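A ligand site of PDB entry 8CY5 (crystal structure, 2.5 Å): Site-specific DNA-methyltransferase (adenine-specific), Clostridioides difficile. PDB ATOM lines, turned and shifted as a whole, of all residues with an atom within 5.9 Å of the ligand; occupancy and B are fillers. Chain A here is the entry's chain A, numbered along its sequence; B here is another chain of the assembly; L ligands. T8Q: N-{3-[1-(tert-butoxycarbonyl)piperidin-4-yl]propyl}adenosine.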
ATOM      1  N   GLY A  29     -22.361  19.518  -3.229  1.00  0.00           N
ATOM      2  CA  GLY A  29     -22.040  19.696  -4.627  1.00  0.00           C
ATOM      3  C   GLY A  29     -21.606  21.106  -4.982  1.00  0.00           C
ATOM      4  O   GLY A  29     -21.839  21.577  -6.092  1.00  0.00           O
ATOM      5  N   ILE A  30     -20.979  21.792  -4.029  1.00  0.00           N
ATOM      6  CA  ILE A  30     -20.475  23.149  -4.215  1.00  0.00           C
ATOM      7  C   ILE A  30     -18.966  23.124  -3.982  1.00  0.00           C
ATOM      8  O   ILE A  30     -18.509  22.786  -2.889  1.00  0.00           O
ATOM      9  CB  ILE A  30     -21.165  24.155  -3.278  1.00  0.00           C
ATOM     10  N   TYR A  31     -18.209  23.490  -5.012  1.00  0.00           N
ATOM     11  CA  TYR A  31     -16.749  23.390  -5.005  1.00  0.00           C
ATOM     12  C   TYR A  31     -16.135  24.774  -5.028  1.00  0.00           C
ATOM     13  O   TYR A  31     -16.483  25.608  -5.882  1.00  0.00           O
ATOM     14  CB  TYR A  31     -16.269  22.565  -6.201  1.00  0.00           C
ATOM     15  CG  TYR A  31     -16.818  21.163  -6.254  1.00  0.00           C
ATOM     16  CD1 TYR A  31     -18.057  20.897  -6.826  1.00  0.00           C
ATOM     17  CD2 TYR A  31     -16.107  20.094  -5.732  1.00  0.00           C
ATOM     18  CE1 TYR A  31     -18.571  19.613  -6.870  1.00  0.00           C
ATOM     19  CE2 TYR A  31     -16.603  18.802  -5.765  1.00  0.00           C
ATOM     20  CZ  TYR A  31     -17.837  18.567  -6.340  1.00  0.00           C
ATOM     21  OH  TYR A  31     -18.347  17.292  -6.385  1.00  0.00           O
ATOM     22  N   ILE A  62     -22.802  31.259 -14.959  1.00  0.00           N
ATOM     23  CA  ILE A  62     -23.970  30.387 -15.046  1.00  0.00           C
ATOM     24  C   ILE A  62     -23.906  29.225 -14.065  1.00  0.00           C
ATOM     25  O   ILE A  62     -24.829  28.399 -14.036  1.00  0.00           O
ATOM     26  CB  ILE A  62     -24.163  29.832 -16.471  1.00  0.00           C
ATOM     27  CG1 ILE A  62     -22.951  29.027 -16.916  1.00  0.00           C
ATOM     28  CG2 ILE A  62     -24.438  30.955 -17.435  1.00  0.00           C
ATOM     29  CD1 ILE A  62     -23.114  28.429 -18.295  1.00  0.00           C
ATOM     30  N   SER A  63     -22.848  29.120 -13.267  1.00  0.00           N
ATOM     31  CA  SER A  63     -22.774  28.191 -12.141  1.00  0.00           C
ATOM     32  C   SER A  63     -22.183  28.918 -10.942  1.00  0.00           C
ATOM     33  O   SER A  63     -21.243  28.453 -10.298  1.00  0.00           O
ATOM     34  CB  SER A  63     -21.982  26.931 -12.500  1.00  0.00           C
ATOM     35  OG  SER A  63     -20.704  27.256 -12.991  1.00  0.00           O
ATOM     36  N   CYS A  64     -22.725  30.103 -10.655  1.00  0.00           N
ATOM     37  CA  CYS A  64     -22.071  31.061  -9.762  1.00  0.00           C
ATOM     38  C   CYS A  64     -21.962  30.582  -8.323  1.00  0.00           C
ATOM     39  O   CYS A  64     -21.111  31.091  -7.582  1.00  0.00           O
ATOM     40  CB  CYS A  64     -22.807  32.401  -9.802  1.00  0.00           C
ATOM     41  SG  CYS A  64     -24.536  32.303  -9.293  1.00  0.00           S
ATOM     42  N   GLY A  65     -22.782  29.629  -7.903  1.00  0.00           N
ATOM     43  CA  GLY A  65     -22.720  29.179  -6.520  1.00  0.00           C
ATOM     44  C   GLY A  65     -23.009  30.323  -5.564  1.00  0.00           C
ATOM     45  O   GLY A  65     -23.979  31.072  -5.727  1.00  0.00           O
ATOM     46  N   CYS A  66     -22.149  30.472  -4.550  1.00  0.00           N
ATOM     47  CA  CYS A  66     -22.290  31.553  -3.591  1.00  0.00           C
ATOM     48  C   CYS A  66     -21.671  32.858  -4.079  1.00  0.00           C
ATOM     49  O   CYS A  66     -21.727  33.863  -3.360  1.00  0.00           O
ATOM     50  CB  CYS A  66     -21.681  31.163  -2.244  1.00  0.00           C
ATOM     51  SG  CYS A  66     -22.681  29.990  -1.313  1.00  0.00           S
ATOM     52  N   ALA A 114     -26.374  32.641 -12.334  1.00  0.00           N
ATOM     53  CA  ALA A 114     -27.332  31.546 -12.367  1.00  0.00           C
ATOM     54  C   ALA A 114     -26.754  30.365 -11.606  1.00  0.00           C
ATOM     55  O   ALA A 114     -25.564  30.088 -11.689  1.00  0.00           O
ATOM     56  CB  ALA A 114     -27.655  31.133 -13.813  1.00  0.00           C
ATOM     57  N   ASP A 115     -27.620  29.679 -10.856  1.00  0.00           N
ATOM     58  CA  ASP A 115     -27.196  28.467 -10.167  1.00  0.00           C
ATOM     59  C   ASP A 115     -28.427  27.647  -9.799  1.00  0.00           C
ATOM     60  O   ASP A 115     -29.464  28.198  -9.449  1.00  0.00           O
ATOM     61  CB  ASP A 115     -26.373  28.791  -8.913  1.00  0.00           C
ATOM     62  CG  ASP A 115     -25.560  27.601  -8.434  1.00  0.00           C
ATOM     63  OD1 ASP A 115     -26.157  26.651  -7.875  1.00  0.00           O
ATOM     64  OD2 ASP A 115     -24.335  27.597  -8.648  1.00  0.00           O
ATOM     65  N   ILE A 116     -28.277  26.320  -9.873  1.00  0.00           N
ATOM     66  CA  ILE A 116     -29.392  25.423  -9.593  1.00  0.00           C
ATOM     67  C   ILE A 116     -29.748  25.416  -8.105  1.00  0.00           C
ATOM     68  O   ILE A 116     -30.888  25.099  -7.750  1.00  0.00           O
ATOM     69  CB  ILE A 116     -29.033  24.007 -10.092  1.00  0.00           C
ATOM     70  CG1 ILE A 116     -30.294  23.142 -10.234  1.00  0.00           C
ATOM     71  CG2 ILE A 116     -28.017  23.340  -9.171  1.00  0.00           C
ATOM     72  CD1 ILE A 116     -31.174  23.540 -11.391  1.00  0.00           C
ATOM     73  N   ASP A 117     -28.808  25.770  -7.233  1.00  0.00           N
ATOM     74  CA  ASP A 117     -28.996  25.686  -5.790  1.00  0.00           C
ATOM     75  C   ASP A 117     -29.664  26.955  -5.276  1.00  0.00           C
ATOM     76  O   ASP A 117     -29.094  28.052  -5.369  1.00  0.00           O
ATOM     77  CB  ASP A 117     -27.657  25.454  -5.087  1.00  0.00           C
ATOM     78  CG  ASP A 117     -27.780  25.356  -3.580  1.00  0.00           C
ATOM     79  OD1 ASP A 117     -28.908  25.113  -3.082  1.00  0.00           O
ATOM     80  OD2 ASP A 117     -26.756  25.527  -2.885  1.00  0.00           O
ATOM     81  N   ALA A 120     -27.733  28.841  -2.425  1.00  0.00           N
ATOM     82  CA  ALA A 120     -26.543  29.560  -2.884  1.00  0.00           C
ATOM     83  C   ALA A 120     -26.912  30.938  -3.428  1.00  0.00           C
ATOM     84  O   ALA A 120     -26.240  31.932  -3.132  1.00  0.00           O
ATOM     85  CB  ALA A 120     -25.805  28.743  -3.941  1.00  0.00           C
ATOM     86  N   CYS A 149     -31.975  28.408 -11.473  1.00  0.00           N
ATOM     87  CA  CYS A 149     -32.445  27.658 -12.635  1.00  0.00           C
ATOM     88  C   CYS A 149     -31.357  26.690 -13.087  1.00  0.00           C
ATOM     89  O   CYS A 149     -30.215  26.757 -12.637  1.00  0.00           O
ATOM     90  CB  CYS A 149     -32.815  28.598 -13.784  1.00  0.00           C
ATOM     91  SG  CYS A 149     -31.375  29.351 -14.579  1.00  0.00           S
ATOM     92  N   ASP A 150     -31.756  25.795 -13.987  1.00  0.00           N
ATOM     93  CA  ASP A 150     -30.809  24.981 -14.744  1.00  0.00           C
ATOM     94  C   ASP A 150     -30.288  25.824 -15.888  1.00  0.00           C
ATOM     95  O   ASP A 150     -31.038  26.167 -16.812  1.00  0.00           O
ATOM     96  CB  ASP A 150     -31.490  23.703 -15.239  1.00  0.00           C
ATOM     97  CG  ASP A 150     -30.532  22.744 -15.928  1.00  0.00           C
ATOM     98  OD1 ASP A 150     -29.485  23.181 -16.452  1.00  0.00           O
ATOM     99  OD2 ASP A 150     -30.832  21.534 -15.953  1.00  0.00           O
ATOM    100  N   SER A 151     -28.993  26.167 -15.857  1.00  0.00           N
ATOM    101  CA  SER A 151     -28.426  27.008 -16.897  1.00  0.00           C
ATOM    102  C   SER A 151     -28.438  26.335 -18.261  1.00  0.00           C
ATOM    103  O   SER A 151     -28.358  27.028 -19.284  1.00  0.00           O
ATOM    104  CB  SER A 151     -26.993  27.404 -16.525  1.00  0.00           C
ATOM    105  OG  SER A 151     -26.975  28.212 -15.357  1.00  0.00           O
ATOM    106  N   LEU A 152     -28.535  25.010 -18.306  1.00  0.00           N
ATOM    107  CA  LEU A 152     -28.595  24.303 -19.577  1.00  0.00           C
ATOM    108  C   LEU A 152     -30.004  24.234 -20.157  1.00  0.00           C
ATOM    109  O   LEU A 152     -30.164  23.822 -21.315  1.00  0.00           O
ATOM    110  CB  LEU A 152     -28.046  22.876 -19.423  1.00  0.00           C
ATOM    111  CG  LEU A 152     -26.580  22.778 -19.003  1.00  0.00           C
ATOM    112  CD1 LEU A 152     -26.127  21.326 -19.031  1.00  0.00           C
ATOM    113  CD2 LEU A 152     -25.705  23.637 -19.893  1.00  0.00           C
ATOM    114  N   ASN A 166     -16.808  28.406 -12.871  1.00  0.00           N
ATOM    115  CA  ASN A 166     -16.362  27.019 -12.726  1.00  0.00           C
ATOM    116  C   ASN A 166     -17.570  26.109 -12.830  1.00  0.00           C
ATOM    117  O   ASN A 166     -18.349  25.985 -11.859  1.00  0.00           O
ATOM    118  CB  ASN A 166     -15.633  26.827 -11.387  1.00  0.00           C
ATOM    119  CG  ASN A 166     -15.154  25.407 -11.176  1.00  0.00           C
ATOM    120  OD1 ASN A 166     -15.059  24.619 -12.120  1.00  0.00           O
ATOM    121  ND2 ASN A 166     -14.841  25.077  -9.928  1.00  0.00           N
ATOM    122  N   PRO A 167     -17.769  25.440 -13.960  1.00  0.00           N
ATOM    123  CA  PRO A 167     -18.987  24.649 -14.169  1.00  0.00           C
ATOM    124  C   PRO A 167     -18.957  23.365 -13.346  1.00  0.00           C
ATOM    125  O   PRO A 167     -17.901  22.977 -12.818  1.00  0.00           O
ATOM    126  CB  PRO A 167     -18.951  24.342 -15.673  1.00  0.00           C
ATOM    127  CG  PRO A 167     -17.484  24.309 -15.986  1.00  0.00           C
ATOM    128  CD  PRO A 167     -16.861  25.381 -15.117  1.00  0.00           C
ATOM    129  N   PRO A 168     -20.086  22.688 -13.192  1.00  0.00           N
ATOM    130  CA  PRO A 168     -20.070  21.358 -12.576  1.00  0.00           C
ATOM    131  C   PRO A 168     -19.452  20.322 -13.502  1.00  0.00           C
ATOM    132  O   PRO A 168     -19.558  20.416 -14.725  1.00  0.00           O
ATOM    133  CB  PRO A 168     -21.546  21.065 -12.318  1.00  0.00           C
ATOM    134  CG  PRO A 168     -22.253  21.833 -13.390  1.00  0.00           C
ATOM    135  CD  PRO A 168     -21.458  23.102 -13.564  1.00  0.00           C
ATOM    136  N   ILE A 170     -19.654  16.279 -14.136  1.00  0.00           N
ATOM    137  CA  ILE A 170     -20.314  15.009 -13.856  1.00  0.00           C
ATOM    138  C   ILE A 170     -20.046  14.059 -15.006  1.00  0.00           C
ATOM    139  O   ILE A 170     -20.406  14.354 -16.162  1.00  0.00           O
ATOM    140  CB  ILE A 170     -21.832  15.170 -13.641  1.00  0.00           C
ATOM    141  CG1 ILE A 170     -22.121  16.225 -12.563  1.00  0.00           C
ATOM    142  CG2 ILE A 170     -22.444  13.846 -13.211  1.00  0.00           C
ATOM    143  CD1 ILE A 170     -23.588  16.393 -12.246  1.00  0.00           C
ATOM    144  N   LYS A 174     -21.922   8.808 -13.069  1.00  0.00           N
ATOM    145  CA  LYS A 174     -22.638   9.513 -12.009  1.00  0.00           C
ATOM    146  C   LYS A 174     -23.796  10.357 -12.523  1.00  0.00           C
ATOM    147  O   LYS A 174     -24.630  10.794 -11.719  1.00  0.00           O
ATOM    148  CB  LYS A 174     -21.662  10.378 -11.224  1.00  0.00           C
ATOM    149  CG  LYS A 174     -20.559   9.590 -10.538  1.00  0.00           C
ATOM    150  CD  LYS A 174     -19.492  10.473  -9.912  1.00  0.00           C
ATOM    151  CE  LYS A 174     -18.378   9.628  -9.289  1.00  0.00           C
ATOM    152  NZ  LYS A 174     -17.278  10.457  -8.707  1.00  0.00           N
ATOM    153  N   LEU A 175     -23.873  10.608 -13.834  1.00  0.00           N
ATOM    154  CA  LEU A 175     -24.933  11.469 -14.356  1.00  0.00           C
ATOM    155  C   LEU A 175     -26.256  10.725 -14.382  1.00  0.00           C
ATOM    156  O   LEU A 175     -26.332   9.558 -14.786  1.00  0.00           O
ATOM    157  CB  LEU A 175     -24.569  11.962 -15.757  1.00  0.00           C
ATOM    158  CG  LEU A 175     -25.408  13.143 -16.247  1.00  0.00           C
ATOM    159  CD1 LEU A 175     -25.491  14.206 -15.173  1.00  0.00           C
ATOM    160  CD2 LEU A 175     -24.831  13.731 -17.531  1.00  0.00           C
ATOM    161  N   GLU A 176     -27.312  11.397 -13.925  1.00  0.00           N
ATOM    162  CA  GLU A 176     -28.634  10.782 -13.886  1.00  0.00           C
ATOM    163  C   GLU A 176     -29.107  10.436 -15.295  1.00  0.00           C
ATOM    164  O   GLU A 176     -28.951  11.235 -16.227  1.00  0.00           O
ATOM    165  CB  GLU A 176     -29.628  11.715 -13.195  1.00  0.00           C
ATOM    166  CG  GLU A 176     -30.887  11.021 -12.711  1.00  0.00           C
ATOM    167  CD  GLU A 176     -32.146  11.590 -13.339  1.00  0.00           C
ATOM    168  OE1 GLU A 176     -32.139  12.785 -13.716  1.00  0.00           O
ATOM    169  OE2 GLU A 176     -33.135  10.826 -13.471  1.00  0.00           O
ATOM    170  N   TYR A 179     -31.608  12.717 -17.203  1.00  0.00           N
ATOM    171  CA  TYR A 179     -30.981  13.953 -17.662  1.00  0.00           C
ATOM    172  C   TYR A 179     -30.096  13.697 -18.888  1.00  0.00           C
ATOM    173  O   TYR A 179     -30.018  14.550 -19.778  1.00  0.00           O
ATOM    174  CB  TYR A 179     -30.168  14.574 -16.534  1.00  0.00           C
ATOM    175  CG  TYR A 179     -29.874  16.046 -16.730  1.00  0.00           C
ATOM    176  CD1 TYR A 179     -28.779  16.472 -17.472  1.00  0.00           C
ATOM    177  CD2 TYR A 179     -30.698  17.026 -16.179  1.00  0.00           C
ATOM    178  CE1 TYR A 179     -28.507  17.811 -17.654  1.00  0.00           C
ATOM    179  CE2 TYR A 179     -30.435  18.370 -16.352  1.00  0.00           C
ATOM    180  CZ  TYR A 179     -29.340  18.751 -17.099  1.00  0.00           C
ATOM    181  OH  TYR A 179     -29.077  20.095 -17.272  1.00  0.00           O
ATOM    182  N   LEU A 197     -20.628  16.382 -18.305  1.00  0.00           N
ATOM    183  CA  LEU A 197     -21.588  17.477 -18.205  1.00  0.00           C
ATOM    184  C   LEU A 197     -20.943  18.816 -18.545  1.00  0.00           C
ATOM    185  O   LEU A 197     -21.568  19.675 -19.180  1.00  0.00           O
ATOM    186  CB  LEU A 197     -22.200  17.522 -16.814  1.00  0.00           C
ATOM    187  CG  LEU A 197     -23.171  18.673 -16.529  1.00  0.00           C
ATOM    188  CD1 LEU A 197     -24.408  18.558 -17.400  1.00  0.00           C
ATOM    189  CD2 LEU A 197     -23.541  18.728 -15.059  1.00  0.00           C
ATOM    190  N   PHE A 201     -21.642  22.875 -20.717  1.00  0.00           N
ATOM    191  CA  PHE A 201     -21.462  24.244 -20.241  1.00  0.00           C
ATOM    192  C   PHE A 201     -20.528  25.014 -21.159  1.00  0.00           C
ATOM    193  O   PHE A 201     -20.733  26.217 -21.385  1.00  0.00           O
ATOM    194  CB  PHE A 201     -20.939  24.242 -18.811  1.00  0.00           C
ATOM    195  CG  PHE A 201     -22.020  24.105 -17.779  1.00  0.00           C
ATOM    196  CD1 PHE A 201     -22.570  22.859 -17.487  1.00  0.00           C
ATOM    197  CD2 PHE A 201     -22.491  25.213 -17.098  1.00  0.00           C
ATOM    198  CE1 PHE A 201     -23.571  22.731 -16.544  1.00  0.00           C
ATOM    199  CE2 PHE A 201     -23.489  25.095 -16.146  1.00  0.00           C
ATOM    200  CZ  PHE A 201     -24.024  23.851 -15.874  1.00  0.00           C
ATOM    201  P    DA B   8     -14.806  11.713 -12.018  1.00  0.00           P
ATOM    202  OP1  DA B   8     -15.452  10.843 -10.997  1.00  0.00           O
ATOM    203  OP2  DA B   8     -15.612  12.246 -13.137  1.00  0.00           O
ATOM    204  O5'  DA B   8     -14.111  12.950 -11.286  1.00  0.00           O
ATOM    205  C5'  DA B   8     -14.800  14.172 -11.140  1.00  0.00           C
ATOM    206  C4'  DA B   8     -14.236  14.955  -9.969  1.00  0.00           C
ATOM    207  O4'  DA B   8     -14.425  16.377 -10.168  1.00  0.00           O
ATOM    208  C3'  DA B   8     -14.872  14.626  -8.616  1.00  0.00           C
ATOM    209  O3'  DA B   8     -13.857  14.538  -7.630  1.00  0.00           O
ATOM    210  C2'  DA B   8     -15.783  15.823  -8.375  1.00  0.00           C
ATOM    211  C1'  DA B   8     -14.974  16.941  -9.005  1.00  0.00           C
ATOM    212  N9   DA B   8     -15.750  18.112  -9.380  1.00  0.00           N
ATOM    213  C8   DA B   8     -17.010  18.129  -9.914  1.00  0.00           C
ATOM    214  N7   DA B   8     -17.456  19.338 -10.160  1.00  0.00           N
ATOM    215  C5   DA B   8     -16.415  20.168  -9.771  1.00  0.00           C
ATOM    216  C6   DA B   8     -16.262  21.571  -9.784  1.00  0.00           C
ATOM    217  N6   DA B   8     -17.204  22.415 -10.219  1.00  0.00           N
ATOM    218  N1   DA B   8     -15.101  22.067  -9.322  1.00  0.00           N
ATOM    219  C2   DA B   8     -14.159  21.224  -8.878  1.00  0.00           C
ATOM    220  N3   DA B   8     -14.189  19.897  -8.828  1.00  0.00           N
ATOM    221  C4   DA B   8     -15.364  19.420  -9.283  1.00  0.00           C
HETATM  222  N1  T8Q L   1     -25.462  22.074 -12.141  1.00  0.00           N
HETATM  223  C7  T8Q L   1     -25.624  24.321 -11.769  1.00  0.00           C
HETATM  224  C8  T8Q L   1     -26.829  25.768 -12.917  1.00  0.00           C
HETATM  225  N2  T8Q L   1     -25.985  25.590 -11.887  1.00  0.00           N
HETATM  226  C9  T8Q L   1     -26.905  23.584 -13.638  1.00  0.00           C
HETATM  227  O1  T8Q L   1     -25.151  24.200  -7.708  1.00  0.00           O
HETATM  228  C1  T8Q L   1     -23.997  23.835  -8.448  1.00  0.00           C
HETATM  229  O5  T8Q L   1     -27.071  13.490 -11.879  1.00  0.00           O
HETATM  230  C5  T8Q L   1     -24.733  22.436 -11.107  1.00  0.00           C
HETATM  231  C6  T8Q L   1     -26.026  23.257 -12.570  1.00  0.00           C
HETATM  232  N3  T8Q L   1     -27.292  24.863 -13.779  1.00  0.00           N
HETATM  233  C4  T8Q L   1     -24.012  24.497  -9.823  1.00  0.00           C
HETATM  234  O4  T8Q L   1     -27.026  14.704  -9.961  1.00  0.00           O
HETATM  235  C3  T8Q L   1     -20.726  23.542  -9.205  1.00  0.00           C
HETATM  236  O3  T8Q L   1     -22.658  24.556 -10.231  1.00  0.00           O
HETATM  237  C2  T8Q L   1     -21.803  24.587  -9.063  1.00  0.00           C
HETATM  238  N4  T8Q L   1     -27.316  22.702 -14.571  1.00  0.00           N
HETATM  239  N   T8Q L   1     -24.774  23.772 -10.837  1.00  0.00           N
HETATM  240  C   T8Q L   1     -22.721  24.431  -7.852  1.00  0.00           C
HETATM  241  O   T8Q L   1     -22.975  25.713  -7.263  1.00  0.00           O
HETATM  242  C10 T8Q L   1     -26.919  21.307 -14.658  1.00  0.00           C
HETATM  243  C11 T8Q L   1     -27.818  20.410 -13.825  1.00  0.00           C
HETATM  244  C12 T8Q L   1     -27.280  18.993 -13.743  1.00  0.00           C
HETATM  245  C13 T8Q L   1     -28.340  17.933 -13.472  1.00  0.00           C
HETATM  246  C14 T8Q L   1     -28.727  17.862 -11.998  1.00  0.00           C
HETATM  247  C15 T8Q L   1     -27.886  16.853 -11.226  1.00  0.00           C
HETATM  248  C16 T8Q L   1     -27.365  14.472 -11.237  1.00  0.00           C
HETATM  249  C17 T8Q L   1     -26.163  13.762  -9.195  1.00  0.00           C
HETATM  250  C18 T8Q L   1     -26.908  12.454  -9.045  1.00  0.00           C
HETATM  251  C19 T8Q L   1     -24.833  13.558  -9.896  1.00  0.00           C
HETATM  252  C20 T8Q L   1     -25.967  14.441  -7.865  1.00  0.00           C
HETATM  253  C21 T8Q L   1     -28.549  15.457 -13.117  1.00  0.00           C
HETATM  254  C22 T8Q L   1     -27.888  16.552 -13.942  1.00  0.00           C
HETATM  255  N5  T8Q L   1     -28.082  15.490 -11.733  1.00  0.00           N
HETATM  256  O2  T8Q L   1     -19.457  24.048  -8.780  1.00  0.00           O
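OD2 of Asp 115 sits at hydrogen-bond distance from N of Gly 65 (2.7 Å). The side-chain carboxylate (OD1) of Asp 115 sits at hydrogen-bond distance from the backbone NH (N) of Asp 117 (2.9 Å). OD1 of Asp 150 sits at hydrogen-bond distance from N of Leu 152, 2.8 Å away. The backbone carbonyl oxygen of Ile 62 is in hydrogen-bond range of the side-chain hydroxyl of Ser 151. N1 of DA 8 of chain B lies within hydrogen-bond range of the side-chain amide nitrogen (ND2) of Asn 166, at 3.1 Å. The backbone carbonyl oxygen (O) of Asn 166 lies within hydrogen-bond range of the side-chain hydroxyl (OG) of Ser 63. The backbone NH (N) of Ser 63 sits at hydrogen-bond distance from the backbone carbonyl oxygen (O) of Ala 114, 3.3 Å away. OD2 of Asp 117 lies within hydrogen-bond range of N of Ala 120, 3.5 Å away.
Residues that only touch the ligand: Gly 29 (3.5 Å), Tyr 31 (3.96 Å), Ile 62 (3.5 Å), Ser 63 (3.4 Å), Gly 65 (3.6 Å), Asp 117 (3.8 Å), Cys 149 (3.5 Å), Asn 166 (3.8 Å), Pro 168 (3.4 Å), Ile 170 (3.9 Å), Lys 174 (3.3 Å), Leu 175 (3.6 Å), Tyr 179 (3.5 Å), Leu 197 (3.97 Å) and Phe 201 (3.7 Å). Of the 28 residues printed, 21 come within 4 Å of the ligand.
O1 of the ligand is in hydrogen-bond range of OD1 of Asp 115, 2.7 Å away. The side-chain carboxylate of Asp 150 lies within hydrogen-bond range of a nitrogen (N4) of the ligand. The backbone NH (N) of Glu 176 sits at hydrogen-bond distance from an oxygen (O5) of the ligand, at 2.9 Å. The backbone NH of Ser 151 lies within hydrogen-bond range of a nitrogen (N3) of the ligand (3.0 Å). N6 of DA 8 of chain B sits at hydrogen-bond distance from an oxygen (O2) of the ligand (3.1 Å). N of Ile 116 is in hydrogen-bond range of N2 of the ligand (3.1 Å).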
